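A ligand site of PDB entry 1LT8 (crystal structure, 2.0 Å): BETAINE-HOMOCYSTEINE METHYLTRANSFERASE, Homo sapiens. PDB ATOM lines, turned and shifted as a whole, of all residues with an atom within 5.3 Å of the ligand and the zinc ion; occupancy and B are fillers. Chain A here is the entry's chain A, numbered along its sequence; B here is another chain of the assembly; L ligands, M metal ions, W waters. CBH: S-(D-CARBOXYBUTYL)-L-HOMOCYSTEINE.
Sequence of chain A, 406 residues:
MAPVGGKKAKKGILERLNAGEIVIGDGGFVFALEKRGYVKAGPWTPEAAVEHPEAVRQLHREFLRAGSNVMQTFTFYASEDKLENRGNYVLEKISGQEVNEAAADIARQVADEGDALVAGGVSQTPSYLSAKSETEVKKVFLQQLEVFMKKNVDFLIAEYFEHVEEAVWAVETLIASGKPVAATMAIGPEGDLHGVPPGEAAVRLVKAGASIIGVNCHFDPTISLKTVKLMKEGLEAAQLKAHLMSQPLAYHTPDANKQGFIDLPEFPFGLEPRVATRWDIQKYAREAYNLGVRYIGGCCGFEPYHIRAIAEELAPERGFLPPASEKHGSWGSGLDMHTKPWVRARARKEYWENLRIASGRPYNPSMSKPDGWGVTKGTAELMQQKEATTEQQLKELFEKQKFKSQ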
ATOM      1  N   GLY A  27       1.262  -0.026 -12.584  1.00  0.00           N
ATOM      2  CA  GLY A  27       1.791   1.039 -13.419  1.00  0.00           C
ATOM      3  C   GLY A  27       0.873   2.104 -14.010  1.00  0.00           C
ATOM      4  O   GLY A  27      -0.178   2.413 -13.450  1.00  0.00           O
ATOM      5  N   GLY A  28       1.311   2.658 -15.149  1.00  0.00           N
ATOM      6  CA  GLY A  28       0.560   3.699 -15.831  1.00  0.00           C
ATOM      7  C   GLY A  28      -0.265   3.114 -16.974  1.00  0.00           C
ATOM      8  O   GLY A  28       0.252   2.898 -18.074  1.00  0.00           O
ATOM      9  N   PHE A  29      -1.539   2.890 -16.700  1.00  0.00           N
ATOM     10  CA  PHE A  29      -2.467   2.306 -17.667  1.00  0.00           C
ATOM     11  C   PHE A  29      -2.742   3.073 -18.947  1.00  0.00           C
ATOM     12  O   PHE A  29      -2.586   2.518 -20.048  1.00  0.00           O
ATOM     13  CB  PHE A  29      -3.807   1.991 -16.995  1.00  0.00           C
ATOM     14  CG  PHE A  29      -3.872   0.618 -16.404  1.00  0.00           C
ATOM     15  CD1 PHE A  29      -3.071   0.278 -15.320  1.00  0.00           C
ATOM     16  CD2 PHE A  29      -4.703  -0.351 -16.965  1.00  0.00           C
ATOM     17  CE1 PHE A  29      -3.082  -1.018 -14.804  1.00  0.00           C
ATOM     18  CE2 PHE A  29      -4.721  -1.650 -16.460  1.00  0.00           C
ATOM     19  CZ  PHE A  29      -3.910  -1.979 -15.377  1.00  0.00           C
ATOM     20  N   VAL A  30      -3.167   4.332 -18.845  1.00  0.00           N
ATOM     21  CA  VAL A  30      -3.492   5.088 -20.057  1.00  0.00           C
ATOM     22  C   VAL A  30      -2.326   5.162 -21.020  1.00  0.00           C
ATOM     23  O   VAL A  30      -2.499   4.977 -22.219  1.00  0.00           O
ATOM     24  CB  VAL A  30      -4.006   6.522 -19.732  1.00  0.00           C
ATOM     25  CG1 VAL A  30      -5.358   6.448 -19.008  1.00  0.00           C
ATOM     26  CG2 VAL A  30      -2.994   7.285 -18.903  1.00  0.00           C
ATOM     27  N   PHE A  31      -1.136   5.434 -20.507  1.00  0.00           N
ATOM     28  CA  PHE A  31       0.043   5.523 -21.355  1.00  0.00           C
ATOM     29  C   PHE A  31       0.406   4.164 -21.930  1.00  0.00           C
ATOM     30  O   PHE A  31       0.755   4.048 -23.098  1.00  0.00           O
ATOM     31  CB  PHE A  31       1.232   6.091 -20.572  1.00  0.00           C
ATOM     32  CG  PHE A  31       1.401   7.582 -20.710  1.00  0.00           C
ATOM     33  CD1 PHE A  31       2.570   8.104 -21.251  1.00  0.00           C
ATOM     34  CD2 PHE A  31       0.410   8.452 -20.294  1.00  0.00           C
ATOM     35  CE1 PHE A  31       2.742   9.472 -21.375  1.00  0.00           C
ATOM     36  CE2 PHE A  31       0.571   9.831 -20.413  1.00  0.00           C
ATOM     37  CZ  PHE A  31       1.744  10.340 -20.953  1.00  0.00           C
ATOM     38  N   GLY A  42      -4.797  12.523 -25.241  1.00  0.00           N
ATOM     39  CA  GLY A  42      -5.566  13.740 -25.356  1.00  0.00           C
ATOM     40  C   GLY A  42      -6.640  13.643 -24.301  1.00  0.00           C
ATOM     41  O   GLY A  42      -6.490  14.192 -23.204  1.00  0.00           O
ATOM     42  N   TRP A  44      -7.518  10.839 -22.953  1.00  0.00           N
ATOM     43  CA  TRP A  44      -7.040   9.768 -22.086  1.00  0.00           C
ATOM     44  C   TRP A  44      -8.169   9.052 -21.319  1.00  0.00           C
ATOM     45  O   TRP A  44      -8.066   8.867 -20.102  1.00  0.00           O
ATOM     46  CB  TRP A  44      -6.059  10.318 -21.051  1.00  0.00           C
ATOM     47  CG  TRP A  44      -4.876  11.056 -21.602  1.00  0.00           C
ATOM     48  CD1 TRP A  44      -4.630  12.408 -21.514  1.00  0.00           C
ATOM     49  CD2 TRP A  44      -3.714  10.490 -22.220  1.00  0.00           C
ATOM     50  NE1 TRP A  44      -3.384  12.703 -22.023  1.00  0.00           N
ATOM     51  CE2 TRP A  44      -2.806  11.546 -22.461  1.00  0.00           C
ATOM     52  CE3 TRP A  44      -3.350   9.175 -22.577  1.00  0.00           C
ATOM     53  CZ2 TRP A  44      -1.553  11.327 -23.055  1.00  0.00           C
ATOM     54  CZ3 TRP A  44      -2.107   8.976 -23.161  1.00  0.00           C
ATOM     55  CH2 TRP A  44      -1.219  10.042 -23.391  1.00  0.00           C
ATOM     56  N   GLN A  72      -5.479  -1.010  -9.687  1.00  0.00           N
ATOM     57  CA  GLN A  72      -6.325   0.191  -9.683  1.00  0.00           C
ATOM     58  C   GLN A  72      -7.368   0.033 -10.776  1.00  0.00           C
ATOM     59  O   GLN A  72      -7.058  -0.465 -11.867  1.00  0.00           O
ATOM     60  CB  GLN A  72      -5.486   1.447  -9.955  1.00  0.00           C
ATOM     61  CG  GLN A  72      -4.588   1.869  -8.817  1.00  0.00           C
ATOM     62  CD  GLN A  72      -3.916   3.221  -9.064  1.00  0.00           C
ATOM     63  OE1 GLN A  72      -4.585   4.202  -9.371  1.00  0.00           O
ATOM     64  NE2 GLN A  72      -2.602   3.257  -8.927  1.00  0.00           N
ATOM     65  N   PHE A  76      -9.607   6.229 -14.694  1.00  0.00           N
ATOM     66  CA  PHE A  76      -9.030   7.562 -14.742  1.00  0.00           C
ATOM     67  C   PHE A  76      -9.839   8.317 -15.795  1.00  0.00           C
ATOM     68  O   PHE A  76     -10.021   7.840 -16.912  1.00  0.00           O
ATOM     69  CB  PHE A  76      -7.547   7.470 -15.150  1.00  0.00           C
ATOM     70  CG  PHE A  76      -6.875   8.810 -15.309  1.00  0.00           C
ATOM     71  CD1 PHE A  76      -6.637   9.334 -16.572  1.00  0.00           C
ATOM     72  CD2 PHE A  76      -6.468   9.531 -14.188  1.00  0.00           C
ATOM     73  CE1 PHE A  76      -5.994  10.563 -16.742  1.00  0.00           C
ATOM     74  CE2 PHE A  76      -5.838  10.772 -14.336  1.00  0.00           C
ATOM     75  CZ  PHE A  76      -5.595  11.283 -15.615  1.00  0.00           C
ATOM     76  N   TYR A  77     -10.341   9.499 -15.435  1.00  0.00           N
ATOM     77  CA  TYR A  77     -11.152  10.274 -16.355  1.00  0.00           C
ATOM     78  C   TYR A  77     -12.396   9.464 -16.724  1.00  0.00           C
ATOM     79  O   TYR A  77     -12.865   9.503 -17.861  1.00  0.00           O
ATOM     80  CB  TYR A  77     -10.360  10.587 -17.641  1.00  0.00           C
ATOM     81  CG  TYR A  77      -9.317  11.672 -17.490  1.00  0.00           C
ATOM     82  CD1 TYR A  77      -9.059  12.270 -16.250  1.00  0.00           C
ATOM     83  CD2 TYR A  77      -8.588  12.114 -18.602  1.00  0.00           C
ATOM     84  CE1 TYR A  77      -8.114  13.283 -16.124  1.00  0.00           C
ATOM     85  CE2 TYR A  77      -7.638  13.121 -18.487  1.00  0.00           C
ATOM     86  CZ  TYR A  77      -7.397  13.707 -17.243  1.00  0.00           C
ATOM     87  OH  TYR A  77      -6.456  14.704 -17.128  1.00  0.00           O
ATOM     88  N   GLU A 159      -6.463  10.345  -6.641  1.00  0.00           N
ATOM     89  CA  GLU A 159      -5.216  10.701  -7.290  1.00  0.00           C
ATOM     90  C   GLU A 159      -5.348  11.770  -8.356  1.00  0.00           C
ATOM     91  O   GLU A 159      -6.445  12.172  -8.742  1.00  0.00           O
ATOM     92  CB  GLU A 159      -4.537   9.477  -7.895  1.00  0.00           C
ATOM     93  CG  GLU A 159      -5.464   8.598  -8.694  1.00  0.00           C
ATOM     94  CD  GLU A 159      -4.701   7.615  -9.563  1.00  0.00           C
ATOM     95  OE1 GLU A 159      -3.711   7.019  -9.078  1.00  0.00           O
ATOM     96  OE2 GLU A 159      -5.105   7.420 -10.726  1.00  0.00           O
ATOM     97  N   TYR A 160      -4.193  12.226  -8.814  1.00  0.00           N
ATOM     98  CA  TYR A 160      -4.115  13.265  -9.836  1.00  0.00           C
ATOM     99  C   TYR A 160      -4.950  14.469  -9.433  1.00  0.00           C
ATOM    100  O   TYR A 160      -6.045  14.691  -9.954  1.00  0.00           O
ATOM    101  CB  TYR A 160      -4.566  12.721 -11.195  1.00  0.00           C
ATOM    102  CG  TYR A 160      -3.940  13.486 -12.343  1.00  0.00           C
ATOM    103  CD1 TYR A 160      -4.698  14.376 -13.108  1.00  0.00           C
ATOM    104  CD2 TYR A 160      -2.585  13.350 -12.628  1.00  0.00           C
ATOM    105  CE1 TYR A 160      -4.105  15.122 -14.130  1.00  0.00           C
ATOM    106  CE2 TYR A 160      -1.988  14.082 -13.649  1.00  0.00           C
ATOM    107  CZ  TYR A 160      -2.761  14.975 -14.398  1.00  0.00           C
ATOM    108  OH  TYR A 160      -2.167  15.700 -15.407  1.00  0.00           O
ATOM    109  N   ASN A 216       1.749  11.636  -7.117  1.00  0.00           N
ATOM    110  CA  ASN A 216       1.713  10.785  -8.300  1.00  0.00           C
ATOM    111  C   ASN A 216       1.782  11.637  -9.567  1.00  0.00           C
ATOM    112  O   ASN A 216       1.287  12.771  -9.598  1.00  0.00           O
ATOM    113  CB  ASN A 216       0.483   9.874  -8.320  1.00  0.00           C
ATOM    114  CG  ASN A 216      -0.774  10.549  -8.899  1.00  0.00           C
ATOM    115  OD1 ASN A 216      -1.361  11.431  -8.280  1.00  0.00           O
ATOM    116  ND2 ASN A 216      -1.180  10.126 -10.091  1.00  0.00           N
ATOM    117  N   CYS A 217       2.446  11.105 -10.583  1.00  0.00           N
ATOM    118  CA  CYS A 217       2.549  11.775 -11.884  1.00  0.00           C
ATOM    119  C   CYS A 217       3.337  13.086 -11.882  1.00  0.00           C
ATOM    120  O   CYS A 217       3.986  13.450 -10.898  1.00  0.00           O
ATOM    121  CB  CYS A 217       1.143  12.008 -12.424  1.00  0.00           C
ATOM    122  SG  CYS A 217       1.034  12.060 -14.245  1.00  0.00           S
ATOM    123  N   HIS A 218       3.296  13.797 -13.017  1.00  0.00           N
ATOM    124  CA  HIS A 218       3.969  15.086 -13.175  1.00  0.00           C
ATOM    125  C   HIS A 218       5.495  15.132 -13.122  1.00  0.00           C
ATOM    126  O   HIS A 218       6.098  15.844 -13.940  1.00  0.00           O
ATOM    127  CB  HIS A 218       3.408  16.085 -12.148  1.00  0.00           C
ATOM    128  CG  HIS A 218       2.171  16.777 -12.600  1.00  0.00           C
ATOM    129  ND1 HIS A 218       1.171  16.159 -13.321  1.00  0.00           N
ATOM    130  CD2 HIS A 218       1.735  18.045 -12.383  1.00  0.00           C
ATOM    131  CE1 HIS A 218       0.181  16.999 -13.534  1.00  0.00           C
ATOM    132  NE2 HIS A 218       0.497  18.152 -12.977  1.00  0.00           N
ATOM    133  N   LEU A 249       6.381   9.443 -12.304  1.00  0.00           N
ATOM    134  CA  LEU A 249       6.463   9.128 -13.721  1.00  0.00           C
ATOM    135  C   LEU A 249       7.675   8.233 -13.873  1.00  0.00           C
ATOM    136  O   LEU A 249       8.585   8.259 -13.025  1.00  0.00           O
ATOM    137  CB  LEU A 249       6.730  10.394 -14.544  1.00  0.00           C
ATOM    138  CG  LEU A 249       5.720  11.530 -14.516  1.00  0.00           C
ATOM    139  CD1 LEU A 249       6.317  12.765 -15.226  1.00  0.00           C
ATOM    140  CD2 LEU A 249       4.435  11.065 -15.185  1.00  0.00           C
ATOM    141  N   PHE A 261       5.521  17.489 -16.225  1.00  0.00           N
ATOM    142  CA  PHE A 261       5.920  17.116 -17.574  1.00  0.00           C
ATOM    143  C   PHE A 261       4.967  17.508 -18.700  1.00  0.00           C
ATOM    144  O   PHE A 261       5.363  17.544 -19.851  1.00  0.00           O
ATOM    145  CB  PHE A 261       6.244  15.618 -17.657  1.00  0.00           C
ATOM    146  CG  PHE A 261       5.039  14.704 -17.750  1.00  0.00           C
ATOM    147  CD1 PHE A 261       5.125  13.493 -18.445  1.00  0.00           C
ATOM    148  CD2 PHE A 261       3.828  15.009 -17.116  1.00  0.00           C
ATOM    149  CE1 PHE A 261       4.050  12.608 -18.516  1.00  0.00           C
ATOM    150  CE2 PHE A 261       2.755  14.133 -17.164  1.00  0.00           C
ATOM    151  CZ  PHE A 261       2.858  12.926 -17.870  1.00  0.00           C
ATOM    152  N   ILE A 262       3.715  17.820 -18.380  1.00  0.00           N
ATOM    153  CA  ILE A 262       2.775  18.197 -19.418  1.00  0.00           C
ATOM    154  C   ILE A 262       3.236  19.429 -20.185  1.00  0.00           C
ATOM    155  O   ILE A 262       3.015  19.532 -21.388  1.00  0.00           O
ATOM    156  CB  ILE A 262       1.362  18.446 -18.831  1.00  0.00           C
ATOM    157  CG1 ILE A 262       0.750  17.102 -18.420  1.00  0.00           C
ATOM    158  CG2 ILE A 262       0.486  19.148 -19.857  1.00  0.00           C
ATOM    159  CD1 ILE A 262      -0.617  17.204 -17.782  1.00  0.00           C
ATOM    160  N   PHE A 267       5.743  16.311 -24.406  1.00  0.00           N
ATOM    161  CA  PHE A 267       4.533  15.651 -23.922  1.00  0.00           C
ATOM    162  C   PHE A 267       3.466  15.706 -25.010  1.00  0.00           C
ATOM    163  O   PHE A 267       3.200  16.780 -25.562  1.00  0.00           O
ATOM    164  CB  PHE A 267       3.969  16.350 -22.680  1.00  0.00           C
ATOM    165  CG  PHE A 267       2.661  15.737 -22.195  1.00  0.00           C
ATOM    166  CD1 PHE A 267       2.668  14.695 -21.268  1.00  0.00           C
ATOM    167  CD2 PHE A 267       1.430  16.194 -22.687  1.00  0.00           C
ATOM    168  CE1 PHE A 267       1.473  14.110 -20.843  1.00  0.00           C
ATOM    169  CE2 PHE A 267       0.228  15.607 -22.273  1.00  0.00           C
ATOM    170  CZ  PHE A 267       0.250  14.570 -21.340  1.00  0.00           C
ATOM    171  N   CYS A 299       3.424   5.827 -12.089  1.00  0.00           N
ATOM    172  CA  CYS A 299       2.357   6.376 -12.888  1.00  0.00           C
ATOM    173  C   CYS A 299       2.753   6.298 -14.355  1.00  0.00           C
ATOM    174  O   CYS A 299       3.412   5.339 -14.766  1.00  0.00           O
ATOM    175  CB  CYS A 299       2.111   7.820 -12.454  1.00  0.00           C
ATOM    176  SG  CYS A 299       0.520   8.457 -12.995  1.00  0.00           S
ATOM    177  N   CYS A 300       2.370   7.302 -15.142  1.00  0.00           N
ATOM    178  CA  CYS A 300       2.695   7.324 -16.567  1.00  0.00           C
ATOM    179  C   CYS A 300       4.130   6.959 -16.890  1.00  0.00           C
ATOM    180  O   CYS A 300       5.062   7.558 -16.367  1.00  0.00           O
ATOM    181  CB  CYS A 300       2.438   8.699 -17.144  1.00  0.00           C
ATOM    182  SG  CYS A 300       0.740   9.207 -16.813  1.00  0.00           S
ATOM    183  N   HIS B 338      -7.210  19.417 -25.732  1.00  0.00           N
ATOM    184  CA  HIS B 338      -6.609  19.473 -24.401  1.00  0.00           C
ATOM    185  C   HIS B 338      -6.814  20.854 -23.784  1.00  0.00           C
ATOM    186  O   HIS B 338      -6.941  21.842 -24.490  1.00  0.00           O
ATOM    187  CB  HIS B 338      -5.106  19.185 -24.485  1.00  0.00           C
ATOM    188  CG  HIS B 338      -4.445  19.001 -23.152  1.00  0.00           C
ATOM    189  ND1 HIS B 338      -4.297  17.765 -22.561  1.00  0.00           N
ATOM    190  CD2 HIS B 338      -3.877  19.887 -22.299  1.00  0.00           C
ATOM    191  CE1 HIS B 338      -3.673  17.900 -21.404  1.00  0.00           C
ATOM    192  NE2 HIS B 338      -3.408  19.180 -21.222  1.00  0.00           N
HETATM  193  O11 CBH L   1      -2.570   4.475 -14.441  1.00  0.00           O
HETATM  194  C12 CBH L   1      -3.067   5.518 -14.927  1.00  0.00           C
HETATM  195  O13 CBH L   1      -3.037   5.849 -16.130  1.00  0.00           O
HETATM  196  C14 CBH L   1      -3.805   6.475 -13.959  1.00  0.00           C
HETATM  197  N15 CBH L   1      -3.997   5.803 -12.662  1.00  0.00           N
HETATM  198  C16 CBH L   1      -3.009   7.774 -13.748  1.00  0.00           C
HETATM  199  C17 CBH L   1      -2.965   8.612 -15.021  1.00  0.00           C
HETATM  200  S18 CBH L   1      -2.173  10.254 -14.801  1.00  0.00           S
HETATM  201  C19 CBH L   1      -2.382  10.854 -16.519  1.00  0.00           C
HETATM  202  C20 CBH L   1      -2.035  12.319 -16.695  1.00  0.00           C
HETATM  203  C21 CBH L   1      -2.561  12.818 -18.042  1.00  0.00           C
HETATM  204  C22 CBH L   1      -2.405  14.321 -18.159  1.00  0.00           C
HETATM  205  C23 CBH L   1      -3.261  14.855 -19.307  1.00  0.00           C
HETATM  206  O25 CBH L   1      -4.454  15.101 -19.052  1.00  0.00           O
HETATM  207  O24 CBH L   1      -2.708  14.994 -20.408  1.00  0.00           O
HETATM  208 ZN    ZN M   1       0.130   9.975 -14.719  1.00  0.00          ZN
HETATM  209  O   HOH W   1      -3.107  10.173 -11.891  1.00  0.00           O
HETATM  210  O   HOH W   2      -6.125   3.676 -13.505  1.00  0.00           O
HETATM  211  O   HOH W   3      -0.541   6.063 -17.445  1.00  0.00           O
HETATM  212  O   HOH W   4      -3.042   2.570 -12.311  1.00  0.00           O
HETATM  213  O   HOH W   5      -6.747  15.839 -20.706  1.00  0.00           O
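The side-chain carboxylate (OE2) of Glu 159 lies within salt-bridge range of a nitrogen (N15) of the ligand, at 2.8 Å.
OH of Tyr 77 is in hydrogen-bond range of O25 of the ligand (2.8 Å).
O24 of the ligand is in hydrogen-bond range of NE1 of Trp 44, at 2.9 Å.
The backbone NH (N) of Phe 29 sits at hydrogen-bond distance from an oxygen (O11) of the ligand (2.9 Å).
The backbone NH of Val 30 sits at hydrogen-bond distance from an oxygen (O13) of the ligand.
N of Gly 28 lies within hydrogen-bond range of O of Cys 299.
The side-chain sulfur (SG) of Cys 299 sits close to the side-chain amide nitrogen (ND2) of Asn 216, at 3.8 Å.
The side-chain amide oxygen of Gln 72 lies close to the side-chain carboxylate of Glu 159 (3.0 Å).
The backbone NH (N) of Tyr 160 is in hydrogen-bond range of the side-chain amide oxygen (OD1) of Asn 216, at 3.0 Å.
O11 of the ligand sits close to O of Gly 27 (3.3 Å).
CA of Gly 28 touches O11 of the ligand (3.5 Å).
Gln 72 touches the ligand.
Phe 76 touches the ligand (CZ to C19, 3.4 Å).
OH of Tyr 160 touches C22 of the ligand, at 3.1 Å.
Ile 262 touches the ligand (CD1 to C22, 3.4 Å).
Phe 267 touches the ligand.
His 338 of chain B touches the ligand.
Hydrophobic or aromatic side chains within 4 Å of the ligand: Phe 29, Val 30, Trp 44, Phe 76, Tyr 77, Tyr 160, Ile 262, Phe 267 and His 338 of chain B.
The nearest printed residue that does not touch the ligand is Gly 42 (4.7 Å).
Three residues have an atom within 4 Å of the zinc ion: Cys 217, Cys 299 and Cys 300.
The nearest printed residue that does not touch the zinc ion is Leu 249 (4.5 Å).
The zinc ion is bound by SG of Cys 300, S18 of the ligand, SG of Cys 217 and SG of Cys 299.
The zinc ion has four donor atoms within binding distance.
Water W4 lies within hydrogen-bond range of an oxygen (O11) of the ligand (2.9 Å), the backbone carbonyl oxygen (O) of Gly 27 (3.1 Å) and the side-chain amide nitrogen (NE2) of Gln 72 (3.5 Å).
Water W5 bridges O25 of the ligand (2.9 Å) and O of Gly 42 (3.0 Å).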
